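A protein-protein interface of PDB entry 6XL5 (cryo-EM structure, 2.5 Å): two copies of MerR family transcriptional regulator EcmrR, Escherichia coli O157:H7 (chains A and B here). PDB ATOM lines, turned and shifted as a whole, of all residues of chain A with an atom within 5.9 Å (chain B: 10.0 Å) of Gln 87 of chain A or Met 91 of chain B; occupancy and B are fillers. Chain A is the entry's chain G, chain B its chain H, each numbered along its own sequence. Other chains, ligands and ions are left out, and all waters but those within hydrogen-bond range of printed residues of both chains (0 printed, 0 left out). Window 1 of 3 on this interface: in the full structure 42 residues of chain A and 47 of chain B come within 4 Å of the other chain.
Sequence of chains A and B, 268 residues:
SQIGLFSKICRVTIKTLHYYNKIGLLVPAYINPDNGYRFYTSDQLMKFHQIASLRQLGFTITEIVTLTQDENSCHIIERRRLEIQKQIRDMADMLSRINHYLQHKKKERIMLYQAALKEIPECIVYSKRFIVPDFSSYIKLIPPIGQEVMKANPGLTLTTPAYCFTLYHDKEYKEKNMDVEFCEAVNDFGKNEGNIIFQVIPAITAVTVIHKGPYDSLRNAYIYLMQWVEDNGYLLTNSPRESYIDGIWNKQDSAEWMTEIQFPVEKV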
ATOM      1  N   ARG A  80      28.903   4.093   4.784  1.00  0.00           N
ATOM      2  CA  ARG A  80      29.065   5.070   3.712  1.00  0.00           C
ATOM      3  C   ARG A  80      27.887   5.040   2.747  1.00  0.00           C
ATOM      4  O   ARG A  80      27.458   6.093   2.271  1.00  0.00           O
ATOM      5  CB  ARG A  80      30.373   4.833   2.960  1.00  0.00           C
ATOM      6  CG  ARG A  80      30.604   5.781   1.791  1.00  0.00           C
ATOM      7  CD  ARG A  80      30.558   7.237   2.236  1.00  0.00           C
ATOM      8  NE  ARG A  80      30.523   8.148   1.097  1.00  0.00           N
ATOM      9  CZ  ARG A  80      30.146   9.420   1.165  1.00  0.00           C
ATOM     10  NH1 ARG A  80      29.767   9.941   2.318  1.00  0.00           N
ATOM     11  NH2 ARG A  80      30.133  10.170   0.074  1.00  0.00           N
ATOM     12  N   LEU A  82      24.678   4.202   3.479  1.00  0.00           N
ATOM     13  CA  LEU A  82      23.545   4.852   4.131  1.00  0.00           C
ATOM     14  C   LEU A  82      23.740   6.357   4.182  1.00  0.00           C
ATOM     15  O   LEU A  82      22.794   7.122   3.949  1.00  0.00           O
ATOM     16  CB  LEU A  82      23.300   4.265   5.527  1.00  0.00           C
ATOM     17  CG  LEU A  82      24.269   4.371   6.706  1.00  0.00           C
ATOM     18  CD1 LEU A  82      24.055   5.648   7.517  1.00  0.00           C
ATOM     19  CD2 LEU A  82      24.154   3.139   7.597  1.00  0.00           C
ATOM     20  N   GLU A  83      24.964   6.803   4.462  1.00  0.00           N
ATOM     21  CA  GLU A  83      25.222   8.232   4.473  1.00  0.00           C
ATOM     22  C   GLU A  83      25.069   8.833   3.083  1.00  0.00           C
ATOM     23  O   GLU A  83      24.612   9.973   2.954  1.00  0.00           O
ATOM     24  CB  GLU A  83      26.615   8.509   5.032  1.00  0.00           C
ATOM     25  CG  GLU A  83      26.941   9.982   5.148  1.00  0.00           C
ATOM     26  CD  GLU A  83      28.423  10.260   5.108  1.00  0.00           C
ATOM     27  OE1 GLU A  83      28.821  11.246   4.454  1.00  0.00           O
ATOM     28  OE2 GLU A  83      29.189   9.502   5.733  1.00  0.00           O
ATOM     29  N   ILE A  84      25.433   8.089   2.036  1.00  0.00           N
ATOM     30  CA  ILE A  84      25.261   8.602   0.682  1.00  0.00           C
ATOM     31  C   ILE A  84      23.784   8.763   0.338  1.00  0.00           C
ATOM     32  O   ILE A  84      23.388   9.784  -0.231  1.00  0.00           O
ATOM     33  CB  ILE A  84      25.975   7.683  -0.324  1.00  0.00           C
ATOM     34  CG1 ILE A  84      27.468   7.971  -0.336  1.00  0.00           C
ATOM     35  CG2 ILE A  84      25.462   7.925  -1.719  1.00  0.00           C
ATOM     36  CD1 ILE A  84      28.244   7.026  -1.196  1.00  0.00           C
ATOM     37  N   GLN A  85      22.941   7.777   0.673  1.00  0.00           N
ATOM     38  CA  GLN A  85      21.511   7.966   0.392  1.00  0.00           C
ATOM     39  C   GLN A  85      20.912   9.088   1.229  1.00  0.00           C
ATOM     40  O   GLN A  85      20.037   9.817   0.750  1.00  0.00           O
ATOM     41  CB  GLN A  85      20.666   6.697   0.525  1.00  0.00           C
ATOM     42  CG  GLN A  85      20.752   5.873   1.762  1.00  0.00           C
ATOM     43  CD  GLN A  85      21.348   4.542   1.424  1.00  0.00           C
ATOM     44  OE1 GLN A  85      21.901   4.375   0.341  1.00  0.00           O
ATOM     45  NE2 GLN A  85      21.198   3.569   2.312  1.00  0.00           N
ATOM     46  N   LYS A  86      21.333   9.217   2.490  1.00  0.00           N
ATOM     47  CA  LYS A  86      20.843  10.317   3.314  1.00  0.00           C
ATOM     48  C   LYS A  86      21.234  11.656   2.702  1.00  0.00           C
ATOM     49  O   LYS A  86      20.416  12.584   2.627  1.00  0.00           O
ATOM     50  CB  LYS A  86      21.371  10.180   4.744  1.00  0.00           C
ATOM     51  CG  LYS A  86      20.809  11.196   5.740  1.00  0.00           C
ATOM     52  CD  LYS A  86      21.726  12.391   5.953  1.00  0.00           C
ATOM     53  CE  LYS A  86      22.982  12.012   6.710  1.00  0.00           C
ATOM     54  NZ  LYS A  86      23.878  13.187   6.884  1.00  0.00           N
ATOM     55  N   GLN A  87      22.488  11.774   2.260  1.00  0.00           N
ATOM     56  CA  GLN A  87      22.936  12.996   1.606  1.00  0.00           C
ATOM     57  C   GLN A  87      22.196  13.217   0.294  1.00  0.00           C
ATOM     58  O   GLN A  87      21.943  14.360  -0.081  1.00  0.00           O
ATOM     59  CB  GLN A  87      24.451  12.924   1.390  1.00  0.00           C
ATOM     60  CG  GLN A  87      25.200  14.256   1.222  1.00  0.00           C
ATOM     61  CD  GLN A  87      24.825  15.044  -0.021  1.00  0.00           C
ATOM     62  OE1 GLN A  87      24.628  14.478  -1.097  1.00  0.00           O
ATOM     63  NE2 GLN A  87      24.725  16.360   0.122  1.00  0.00           N
ATOM     64  N   ILE A  88      21.808  12.144  -0.396  1.00  0.00           N
ATOM     65  CA  ILE A  88      21.030  12.289  -1.626  1.00  0.00           C
ATOM     66  C   ILE A  88      19.637  12.830  -1.318  1.00  0.00           C
ATOM     67  O   ILE A  88      19.124  13.699  -2.035  1.00  0.00           O
ATOM     68  CB  ILE A  88      20.984  10.956  -2.391  1.00  0.00           C
ATOM     69  CG1 ILE A  88      22.326  10.711  -3.083  1.00  0.00           C
ATOM     70  CG2 ILE A  88      19.860  10.948  -3.415  1.00  0.00           C
ATOM     71  CD1 ILE A  88      22.345   9.506  -3.980  1.00  0.00           C
ATOM     72  N   ARG A  89      19.000  12.320  -0.259  1.00  0.00           N
ATOM     73  CA  ARG A  89      17.713  12.872   0.162  1.00  0.00           C
ATOM     74  C   ARG A  89      17.849  14.349   0.514  1.00  0.00           C
ATOM     75  O   ARG A  89      17.043  15.180   0.074  1.00  0.00           O
ATOM     76  CB  ARG A  89      17.137  12.097   1.350  1.00  0.00           C
ATOM     77  CG  ARG A  89      16.533  10.750   0.996  1.00  0.00           C
ATOM     78  CD  ARG A  89      15.919  10.061   2.213  1.00  0.00           C
ATOM     79  NE  ARG A  89      16.819   9.932   3.354  1.00  0.00           N
ATOM     80  CZ  ARG A  89      17.471   8.817   3.666  1.00  0.00           C
ATOM     81  NH1 ARG A  89      18.267   8.785   4.726  1.00  0.00           N
ATOM     82  NH2 ARG A  89      17.328   7.733   2.918  1.00  0.00           N
ATOM     83  N   ASP A  90      18.897  14.695   1.265  1.00  0.00           N
ATOM     84  CA  ASP A  90      19.104  16.081   1.672  1.00  0.00           C
ATOM     85  C   ASP A  90      19.396  16.956   0.466  1.00  0.00           C
ATOM     86  O   ASP A  90      18.986  18.121   0.415  1.00  0.00           O
ATOM     87  CB  ASP A  90      20.255  16.190   2.668  1.00  0.00           C
ATOM     88  CG  ASP A  90      20.032  15.370   3.910  1.00  0.00           C
ATOM     89  OD1 ASP A  90      18.921  14.830   4.074  1.00  0.00           O
ATOM     90  OD2 ASP A  90      20.965  15.284   4.730  1.00  0.00           O
ATOM     91  N   MET A  91      20.088  16.399  -0.521  1.00  0.00           N
ATOM     92  CA  MET A  91      20.442  17.145  -1.714  1.00  0.00           C
ATOM     93  C   MET A  91      19.224  17.386  -2.587  1.00  0.00           C
ATOM     94  O   MET A  91      19.099  18.445  -3.205  1.00  0.00           O
ATOM     95  CB  MET A  91      21.504  16.374  -2.486  1.00  0.00           C
ATOM     96  CG  MET A  91      22.471  17.258  -3.187  1.00  0.00           C
ATOM     97  SD  MET A  91      23.602  17.804  -1.905  1.00  0.00           S
ATOM     98  CE  MET A  91      24.810  18.657  -2.879  1.00  0.00           C
ATOM     99  N   ALA A  92      18.328  16.406  -2.671  1.00  0.00           N
ATOM    100  CA  ALA A  92      17.075  16.628  -3.381  1.00  0.00           C
ATOM    101  C   ALA A  92      16.232  17.688  -2.683  1.00  0.00           C
ATOM    102  O   ALA A  92      15.613  18.533  -3.345  1.00  0.00           O
ATOM    103  CB  ALA A  92      16.304  15.317  -3.505  1.00  0.00           C
ATOM    104  N   GLN B  56      20.853  26.917   5.037  1.00  0.00           N
ATOM    105  CA  GLN B  56      20.174  25.646   4.823  1.00  0.00           C
ATOM    106  C   GLN B  56      20.038  25.295   3.341  1.00  0.00           C
ATOM    107  O   GLN B  56      19.682  24.159   3.014  1.00  0.00           O
ATOM    108  CB  GLN B  56      18.827  25.663   5.536  1.00  0.00           C
ATOM    109  CG  GLN B  56      18.316  24.277   5.846  1.00  0.00           C
ATOM    110  CD  GLN B  56      16.969  24.276   6.514  1.00  0.00           C
ATOM    111  OE1 GLN B  56      16.299  25.304   6.600  1.00  0.00           O
ATOM    112  NE2 GLN B  56      16.582  23.120   7.038  1.00  0.00           N
ATOM    113  N   LEU B  57      20.329  26.233   2.447  1.00  0.00           N
ATOM    114  CA  LEU B  57      20.311  26.002   1.010  1.00  0.00           C
ATOM    115  C   LEU B  57      21.680  25.618   0.476  1.00  0.00           C
ATOM    116  O   LEU B  57      21.816  25.385  -0.728  1.00  0.00           O
ATOM    117  CB  LEU B  57      19.793  27.243   0.274  1.00  0.00           C
ATOM    118  CG  LEU B  57      18.316  27.276  -0.122  1.00  0.00           C
ATOM    119  CD1 LEU B  57      17.413  26.887   1.028  1.00  0.00           C
ATOM    120  CD2 LEU B  57      17.949  28.672  -0.608  1.00  0.00           C
ATOM    121  N   GLY B  58      22.696  25.575   1.332  1.00  0.00           N
ATOM    122  CA  GLY B  58      24.021  25.159   0.934  1.00  0.00           C
ATOM    123  C   GLY B  58      24.992  26.266   0.611  1.00  0.00           C
ATOM    124  O   GLY B  58      26.143  25.966   0.271  1.00  0.00           O
ATOM    125  N   ARG B  80      24.678  28.270  -7.857  1.00  0.00           N
ATOM    126  CA  ARG B  80      24.588  27.272  -6.796  1.00  0.00           C
ATOM    127  C   ARG B  80      23.710  26.095  -7.205  1.00  0.00           C
ATOM    128  O   ARG B  80      23.985  24.953  -6.822  1.00  0.00           O
ATOM    129  CB  ARG B  80      24.049  27.924  -5.517  1.00  0.00           C
ATOM    130  CG  ARG B  80      23.722  26.960  -4.380  1.00  0.00           C
ATOM    131  CD  ARG B  80      24.949  26.285  -3.824  1.00  0.00           C
ATOM    132  NE  ARG B  80      24.607  25.069  -3.093  1.00  0.00           N
ATOM    133  CZ  ARG B  80      25.502  24.194  -2.651  1.00  0.00           C
ATOM    134  NH1 ARG B  80      25.114  23.112  -1.998  1.00  0.00           N
ATOM    135  NH2 ARG B  80      26.793  24.410  -2.853  1.00  0.00           N
ATOM    136  N   GLU B  83      25.794  23.892  -9.464  1.00  0.00           N
ATOM    137  CA  GLU B  83      26.787  23.228  -8.624  1.00  0.00           C
ATOM    138  C   GLU B  83      26.175  22.078  -7.818  1.00  0.00           C
ATOM    139  O   GLU B  83      26.762  20.990  -7.732  1.00  0.00           O
ATOM    140  CB  GLU B  83      27.444  24.284  -7.734  1.00  0.00           C
ATOM    141  CG  GLU B  83      28.705  23.868  -7.010  1.00  0.00           C
ATOM    142  CD  GLU B  83      28.452  23.299  -5.643  1.00  0.00           C
ATOM    143  OE1 GLU B  83      27.572  23.815  -4.930  1.00  0.00           O
ATOM    144  OE2 GLU B  83      29.173  22.362  -5.266  1.00  0.00           O
ATOM    145  N   ILE B  84      24.985  22.287  -7.242  1.00  0.00           N
ATOM    146  CA  ILE B  84      24.321  21.210  -6.506  1.00  0.00           C
ATOM    147  C   ILE B  84      23.916  20.090  -7.457  1.00  0.00           C
ATOM    148  O   ILE B  84      23.963  18.912  -7.095  1.00  0.00           O
ATOM    149  CB  ILE B  84      23.141  21.701  -5.637  1.00  0.00           C
ATOM    150  CG1 ILE B  84      22.558  20.522  -4.866  1.00  0.00           C
ATOM    151  CG2 ILE B  84      22.034  22.303  -6.416  1.00  0.00           C
ATOM    152  CD1 ILE B  84      21.521  20.877  -3.886  1.00  0.00           C
ATOM    153  N   GLN B  85      23.468  20.434  -8.669  1.00  0.00           N
ATOM    154  CA  GLN B  85      23.117  19.404  -9.641  1.00  0.00           C
ATOM    155  C   GLN B  85      24.326  18.551 -10.002  1.00  0.00           C
ATOM    156  O   GLN B  85      24.218  17.323 -10.124  1.00  0.00           O
ATOM    157  CB  GLN B  85      22.519  20.046 -10.888  1.00  0.00           C
ATOM    158  CG  GLN B  85      21.111  20.563 -10.693  1.00  0.00           C
ATOM    159  CD  GLN B  85      20.507  21.095 -11.969  1.00  0.00           C
ATOM    160  OE1 GLN B  85      21.187  21.212 -12.987  1.00  0.00           O
ATOM    161  NE2 GLN B  85      19.223  21.425 -11.924  1.00  0.00           N
ATOM    162  N   LYS B  86      25.491  19.175 -10.172  1.00  0.00           N
ATOM    163  CA  LYS B  86      26.684  18.383 -10.437  1.00  0.00           C
ATOM    164  C   LYS B  86      27.026  17.490  -9.249  1.00  0.00           C
ATOM    165  O   LYS B  86      27.325  16.300  -9.423  1.00  0.00           O
ATOM    166  CB  LYS B  86      27.844  19.326 -10.751  1.00  0.00           C
ATOM    167  CG  LYS B  86      29.151  18.668 -11.126  1.00  0.00           C
ATOM    168  CD  LYS B  86      30.205  19.732 -11.415  1.00  0.00           C
ATOM    169  CE  LYS B  86      31.494  19.118 -11.934  1.00  0.00           C
ATOM    170  NZ  LYS B  86      32.186  18.300 -10.901  1.00  0.00           N
ATOM    171  N   GLN B  87      26.913  18.027  -8.026  1.00  0.00           N
ATOM    172  CA  GLN B  87      27.198  17.217  -6.841  1.00  0.00           C
ATOM    173  C   GLN B  87      26.212  16.066  -6.665  1.00  0.00           C
ATOM    174  O   GLN B  87      26.606  14.971  -6.262  1.00  0.00           O
ATOM    175  CB  GLN B  87      27.249  18.074  -5.577  1.00  0.00           C
ATOM    176  CG  GLN B  87      28.427  19.038  -5.520  1.00  0.00           C
ATOM    177  CD  GLN B  87      28.583  19.698  -4.161  1.00  0.00           C
ATOM    178  OE1 GLN B  87      27.776  19.501  -3.260  1.00  0.00           O
ATOM    179  NE2 GLN B  87      29.642  20.481  -4.009  1.00  0.00           N
ATOM    180  N   ILE B  88      24.926  16.293  -6.940  1.00  0.00           N
ATOM    181  CA  ILE B  88      23.943  15.215  -6.825  1.00  0.00           C
ATOM    182  C   ILE B  88      24.191  14.146  -7.882  1.00  0.00           C
ATOM    183  O   ILE B  88      24.052  12.949  -7.604  1.00  0.00           O
ATOM    184  CB  ILE B  88      22.488  15.740  -6.821  1.00  0.00           C
ATOM    185  CG1 ILE B  88      21.517  14.606  -6.481  1.00  0.00           C
ATOM    186  CG2 ILE B  88      22.060  16.335  -8.128  1.00  0.00           C
ATOM    187  CD1 ILE B  88      21.844  13.876  -5.194  1.00  0.00           C
ATOM    188  N   ARG B  89      24.511  14.545  -9.120  1.00  0.00           N
ATOM    189  CA  ARG B  89      24.764  13.544 -10.151  1.00  0.00           C
ATOM    190  C   ARG B  89      25.999  12.719  -9.808  1.00  0.00           C
ATOM    191  O   ARG B  89      26.007  11.491  -9.996  1.00  0.00           O
ATOM    192  CB  ARG B  89      24.921  14.232 -11.502  1.00  0.00           C
ATOM    193  CG  ARG B  89      24.951  13.301 -12.686  1.00  0.00           C
ATOM    194  CD  ARG B  89      24.891  14.094 -13.980  1.00  0.00           C
ATOM    195  NE  ARG B  89      25.742  15.279 -13.934  1.00  0.00           N
ATOM    196  CZ  ARG B  89      25.295  16.525 -14.037  1.00  0.00           C
ATOM    197  NH1 ARG B  89      24.000  16.758 -14.196  1.00  0.00           N
ATOM    198  NH2 ARG B  89      26.145  17.540 -13.983  1.00  0.00           N
ATOM    199  N   ASP B  90      26.961  13.335  -9.117  1.00  0.00           N
ATOM    200  CA  ASP B  90      28.135  12.591  -8.681  1.00  0.00           C
ATOM    201  C   ASP B  90      27.793  11.713  -7.487  1.00  0.00           C
ATOM    202  O   ASP B  90      28.344  10.619  -7.350  1.00  0.00           O
ATOM    203  CB  ASP B  90      29.285  13.537  -8.351  1.00  0.00           C
ATOM    204  CG  ASP B  90      29.680  14.403  -9.529  1.00  0.00           C
ATOM    205  OD1 ASP B  90      29.064  14.255 -10.603  1.00  0.00           O
ATOM    206  OD2 ASP B  90      30.611  15.223  -9.387  1.00  0.00           O
ATOM    207  N   MET B  91      26.917  12.181  -6.599  1.00  0.00           N
ATOM    208  CA  MET B  91      26.572  11.389  -5.425  1.00  0.00           C
ATOM    209  C   MET B  91      25.776  10.162  -5.841  1.00  0.00           C
ATOM    210  O   MET B  91      25.940   9.084  -5.262  1.00  0.00           O
ATOM    211  CB  MET B  91      25.761  12.227  -4.436  1.00  0.00           C
ATOM    212  CG  MET B  91      26.559  13.179  -3.575  1.00  0.00           C
ATOM    213  SD  MET B  91      27.819  12.380  -2.572  1.00  0.00           S
ATOM    214  CE  MET B  91      29.122  13.599  -2.683  1.00  0.00           C
ATOM    215  N   ALA B  92      24.886  10.320  -6.825  1.00  0.00           N
ATOM    216  CA  ALA B  92      24.153   9.180  -7.363  1.00  0.00           C
ATOM    217  C   ALA B  92      25.100   8.202  -8.045  1.00  0.00           C
ATOM    218  O   ALA B  92      24.941   6.977  -7.926  1.00  0.00           O
ATOM    219  CB  ALA B  92      23.077   9.659  -8.335  1.00  0.00           C
ATOM    220  N   ASP B  93      26.108   8.729  -8.753  1.00  0.00           N
ATOM    221  CA  ASP B  93      27.141   7.867  -9.320  1.00  0.00           C
ATOM    222  C   ASP B  93      27.849   7.075  -8.223  1.00  0.00           C
ATOM    223  O   ASP B  93      27.985   5.851  -8.317  1.00  0.00           O
ATOM    224  CB  ASP B  93      28.129   8.707 -10.129  1.00  0.00           C
ATOM    225  CG  ASP B  93      29.247   7.879 -10.725  1.00  0.00           C
ATOM    226  OD1 ASP B  93      30.405   8.345 -10.709  1.00  0.00           O
ATOM    227  OD2 ASP B  93      28.970   6.762 -11.210  1.00  0.00           O
ATOM    228  N   MET B  94      28.299   7.769  -7.172  1.00  0.00           N
ATOM    229  CA  MET B  94      28.960   7.122  -6.040  1.00  0.00           C
ATOM    230  C   MET B  94      28.057   6.082  -5.386  1.00  0.00           C
ATOM    231  O   MET B  94      28.536   5.057  -4.890  1.00  0.00           O
ATOM    232  CB  MET B  94      29.402   8.166  -5.017  1.00  0.00           C
ATOM    233  CG  MET B  94      30.560   9.039  -5.466  1.00  0.00           C
ATOM    234  SD  MET B  94      31.030  10.259  -4.224  1.00  0.00           S
ATOM    235  CE  MET B  94      31.103  11.746  -5.214  1.00  0.00           C
ATOM    236  N   LEU B  95      26.751   6.346  -5.341  1.00  0.00           N
ATOM    237  CA  LEU B  95      25.815   5.391  -4.754  1.00  0.00           C
ATOM    238  C   LEU B  95      25.740   4.121  -5.585  1.00  0.00           C
ATOM    239  O   LEU B  95      25.717   3.007  -5.041  1.00  0.00           O
ATOM    240  CB  LEU B  95      24.429   6.012  -4.631  1.00  0.00           C
ATOM    241  CG  LEU B  95      23.419   5.118  -3.915  1.00  0.00           C
ATOM    242  CD1 LEU B  95      23.955   4.650  -2.567  1.00  0.00           C
ATOM    243  CD2 LEU B  95      22.096   5.838  -3.764  1.00  0.00           C
ATOM    244  N   SER B  96      25.680   4.270  -6.907  1.00  0.00           N
ATOM    245  CA  SER B  96      25.694   3.091  -7.761  1.00  0.00           C
ATOM    246  C   SER B  96      27.004   2.332  -7.603  1.00  0.00           C
ATOM    247  O   SER B  96      27.020   1.095  -7.557  1.00  0.00           O
ATOM    248  CB  SER B  96      25.477   3.497  -9.214  1.00  0.00           C
ATOM    249  OG  SER B  96      26.279   4.616  -9.539  1.00  0.00           O
ATOM    250  N   ARG B  97      28.110   3.059  -7.452  1.00  0.00           N
ATOM    251  CA  ARG B  97      29.392   2.386  -7.287  1.00  0.00           C
ATOM    252  C   ARG B  97      29.486   1.637  -5.958  1.00  0.00           C
ATOM    253  O   ARG B  97      30.007   0.521  -5.919  1.00  0.00           O
ATOM    254  CB  ARG B  97      30.517   3.418  -7.391  1.00  0.00           C
ATOM    255  CG  ARG B  97      30.581   4.193  -8.702  1.00  0.00           C
ATOM    256  CD  ARG B  97      31.684   3.715  -9.619  1.00  0.00           C
ATOM    257  NE  ARG B  97      33.009   4.031  -9.094  1.00  0.00           N
ATOM    258  CZ  ARG B  97      33.589   5.221  -9.199  1.00  0.00           C
ATOM    259  NH1 ARG B  97      32.961   6.218  -9.804  1.00  0.00           N
ATOM    260  NH2 ARG B  97      34.796   5.419  -8.694  1.00  0.00           N
ATOM    261  N   ILE B  98      28.988   2.220  -4.860  1.00  0.00           N
ATOM    262  CA  ILE B  98      29.027   1.514  -3.577  1.00  0.00           C
ATOM    263  C   ILE B  98      28.081   0.307  -3.541  1.00  0.00           C
ATOM    264  O   ILE B  98      28.430  -0.738  -2.973  1.00  0.00           O
ATOM    265  CB  ILE B  98      28.801   2.486  -2.400  1.00  0.00           C
ATOM    266  CG1 ILE B  98      28.995   1.768  -1.062  1.00  0.00           C
ATOM    267  CG2 ILE B  98      27.453   3.137  -2.444  1.00  0.00           C
ATOM    268  CD1 ILE B  98      30.356   1.138  -0.899  1.00  0.00           C
ATOM    269  N   ASN B  99      26.870   0.414  -4.116  1.00  0.00           N
ATOM    270  CA  ASN B  99      26.002  -0.771  -4.163  1.00  0.00           C
ATOM    271  C   ASN B  99      26.657  -1.874  -4.990  1.00  0.00           C
ATOM    272  O   ASN B  99      26.586  -3.057  -4.635  1.00  0.00           O
ATOM    273  CB  ASN B  99      24.558  -0.467  -4.601  1.00  0.00           C
ATOM    274  CG  ASN B  99      24.432   0.114  -5.975  1.00  0.00           C
ATOM    275  OD1 ASN B  99      24.942  -0.433  -6.947  1.00  0.00           O
ATOM    276  ND2 ASN B  99      23.662   1.190  -6.080  1.00  0.00           N
ATOM    277  N   TYR B 234      27.430   2.755 -17.138  1.00  0.00           N
ATOM    278  CA  TYR B 234      28.408   3.354 -18.030  1.00  0.00           C
ATOM    279  C   TYR B 234      28.323   2.745 -19.426  1.00  0.00           C
ATOM    280  O   TYR B 234      27.667   1.727 -19.658  1.00  0.00           O
ATOM    281  CB  TYR B 234      29.809   3.192 -17.444  1.00  0.00           C
ATOM    282  CG  TYR B 234      30.193   4.247 -16.430  1.00  0.00           C
ATOM    283  CD1 TYR B 234      29.770   4.159 -15.110  1.00  0.00           C
ATOM    284  CD2 TYR B 234      30.989   5.325 -16.791  1.00  0.00           C
ATOM    285  CE1 TYR B 234      30.127   5.120 -14.182  1.00  0.00           C
ATOM    286  CE2 TYR B 234      31.351   6.289 -15.875  1.00  0.00           C
ATOM    287  CZ  TYR B 234      30.917   6.184 -14.571  1.00  0.00           C
ATOM    288  OH  TYR B 234      31.274   7.146 -13.654  1.00  0.00           O
ATOM    289  N   LYS B 267      29.473   8.006 -18.656  1.00  0.00           N
ATOM    290  CA  LYS B 267      28.317   7.586 -17.881  1.00  0.00           C
ATOM    291  C   LYS B 267      27.027   7.902 -18.620  1.00  0.00           C
ATOM    292  O   LYS B 267      26.907   8.937 -19.282  1.00  0.00           O
ATOM    293  CB  LYS B 267      28.301   8.247 -16.506  1.00  0.00           C
ATOM    294  CG  LYS B 267      27.503   7.453 -15.483  1.00  0.00           C
ATOM    295  CD  LYS B 267      27.676   8.006 -14.090  1.00  0.00           C
ATOM    296  CE  LYS B 267      26.935   9.318 -13.937  1.00  0.00           C
ATOM    297  NZ  LYS B 267      25.460   9.117 -13.980  1.00  0.00           N
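Met 91 of chain B touches Ile 84 of chain A.
Ile 84 of chain A touches Leu 95 of chain B (CG2 to CB, 3.6 Å).
Leu 95 of chain B touches Gln 85 of chain A.
Met 91 of chain B touches Gln 87 of chain A (CG to OE1, 3.4 Å).
Ile 88 of chain B touches Ile 88 of chain A (CD1 to CG1, 3.8 Å).
O of Met 91 of chain B touches CD1 of Ile 88 of chain A (3.8 Å).
Ile 88 of chain A touches Leu 95 of chain B (CD1 to CD2, 3.7 Å).
Ile 84 of chain B touches Met 91 of chain A.
Met 91 of chain A touches Gln 87 of chain B.
Ile 88 of chain B touches Met 91 of chain A (CD1 to CB, 3.7 Å).
Gln 87 of chain A touches one residue of chain B.
Of chain A, only Ile 84, Gln 87 and Ile 88 come within 4 Å of Met 91 of chain B.
No residue of chain B comes within 4 Å of Lys 86 of chain A.
Ile 88 of chain A touches four residues of chain B.
No residue of chain B comes within 4 Å of Asp 90 of chain A.
Of the printed residues of chain B, Met 91 of chain A touches Ile 84, Gln 87 and Ile 88.
Printed residues of chain A within 4 Å of Leu 95 of chain B: Ile 84, Gln 85 and Ile 88.
Of the printed residues of chain A, Gln 87 of chain B touches Met 91 (3.1 Å).
Of the printed residues of chain A, Ile 88 of chain B touches Ile 88 (3.8 Å) and Met 91 (3.7 Å).
Printed residues of chain B within 4 Å of Gln 85 of chain A: Leu 95 (3.6 Å).
Printed residues of chain A within 4 Å of Ile 84 of chain B: Met 91.
Arg 89 of chain A touches none of the printed residues of chain B.
Ser 96 of chain B touches none of the printed residues of chain A.
The nearest residue of chain A that does not touch Met 91 of chain B is Arg 80 of chain A (4.2 Å).
The nearest printed residue of chain A that does not touch Ile 88 of chain B is Gln 87 of chain A (5.0 Å).
Ile 84 of chain A touches Met 91 of chain B, and with the chains exchanged Met 91 of chain A touches Ile 84 of chain B.
Ile 88 of chain B touches its own counterpart, Ile 88 of chain A.
Ile 88 of chain A touches Met 91 of chain B, and with the chains exchanged Met 91 of chain A touches Ile 88 of chain B.
Ile 88 of chain A touches Ala 92 of chain B, but with the chains exchanged Ala 92 of chain A does not touch Ile 88 of chain B (5.0 Å).
Positions printed for both chains: 80, 83, 84, 85, 86, 87, 88, 89, 90, 91 and 92.
NE2 of Gln 87 of chain A is in hydrogen-bond range of SD of Met 91 of chain A, at 2.7 Å.
OG of Ser 96 of chain B is in hydrogen-bond range of O of Ala 92 of chain B, at 3.2 Å.
O of Leu 95 of chain B lies within hydrogen-bond range of ND2 of Asn 99 of chain B, at 2.9 Å.
Of the 23 printed residues of chain B, 6 touch a printed residue of chain A.
Printed residues of chain A that touch a printed residue of chain B: Ile 84, Gln 85, Gln 87, Ile 88 and Met 91.
Along chain A the printed residues that touch a printed residue of chain B span positions 84 to 91.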
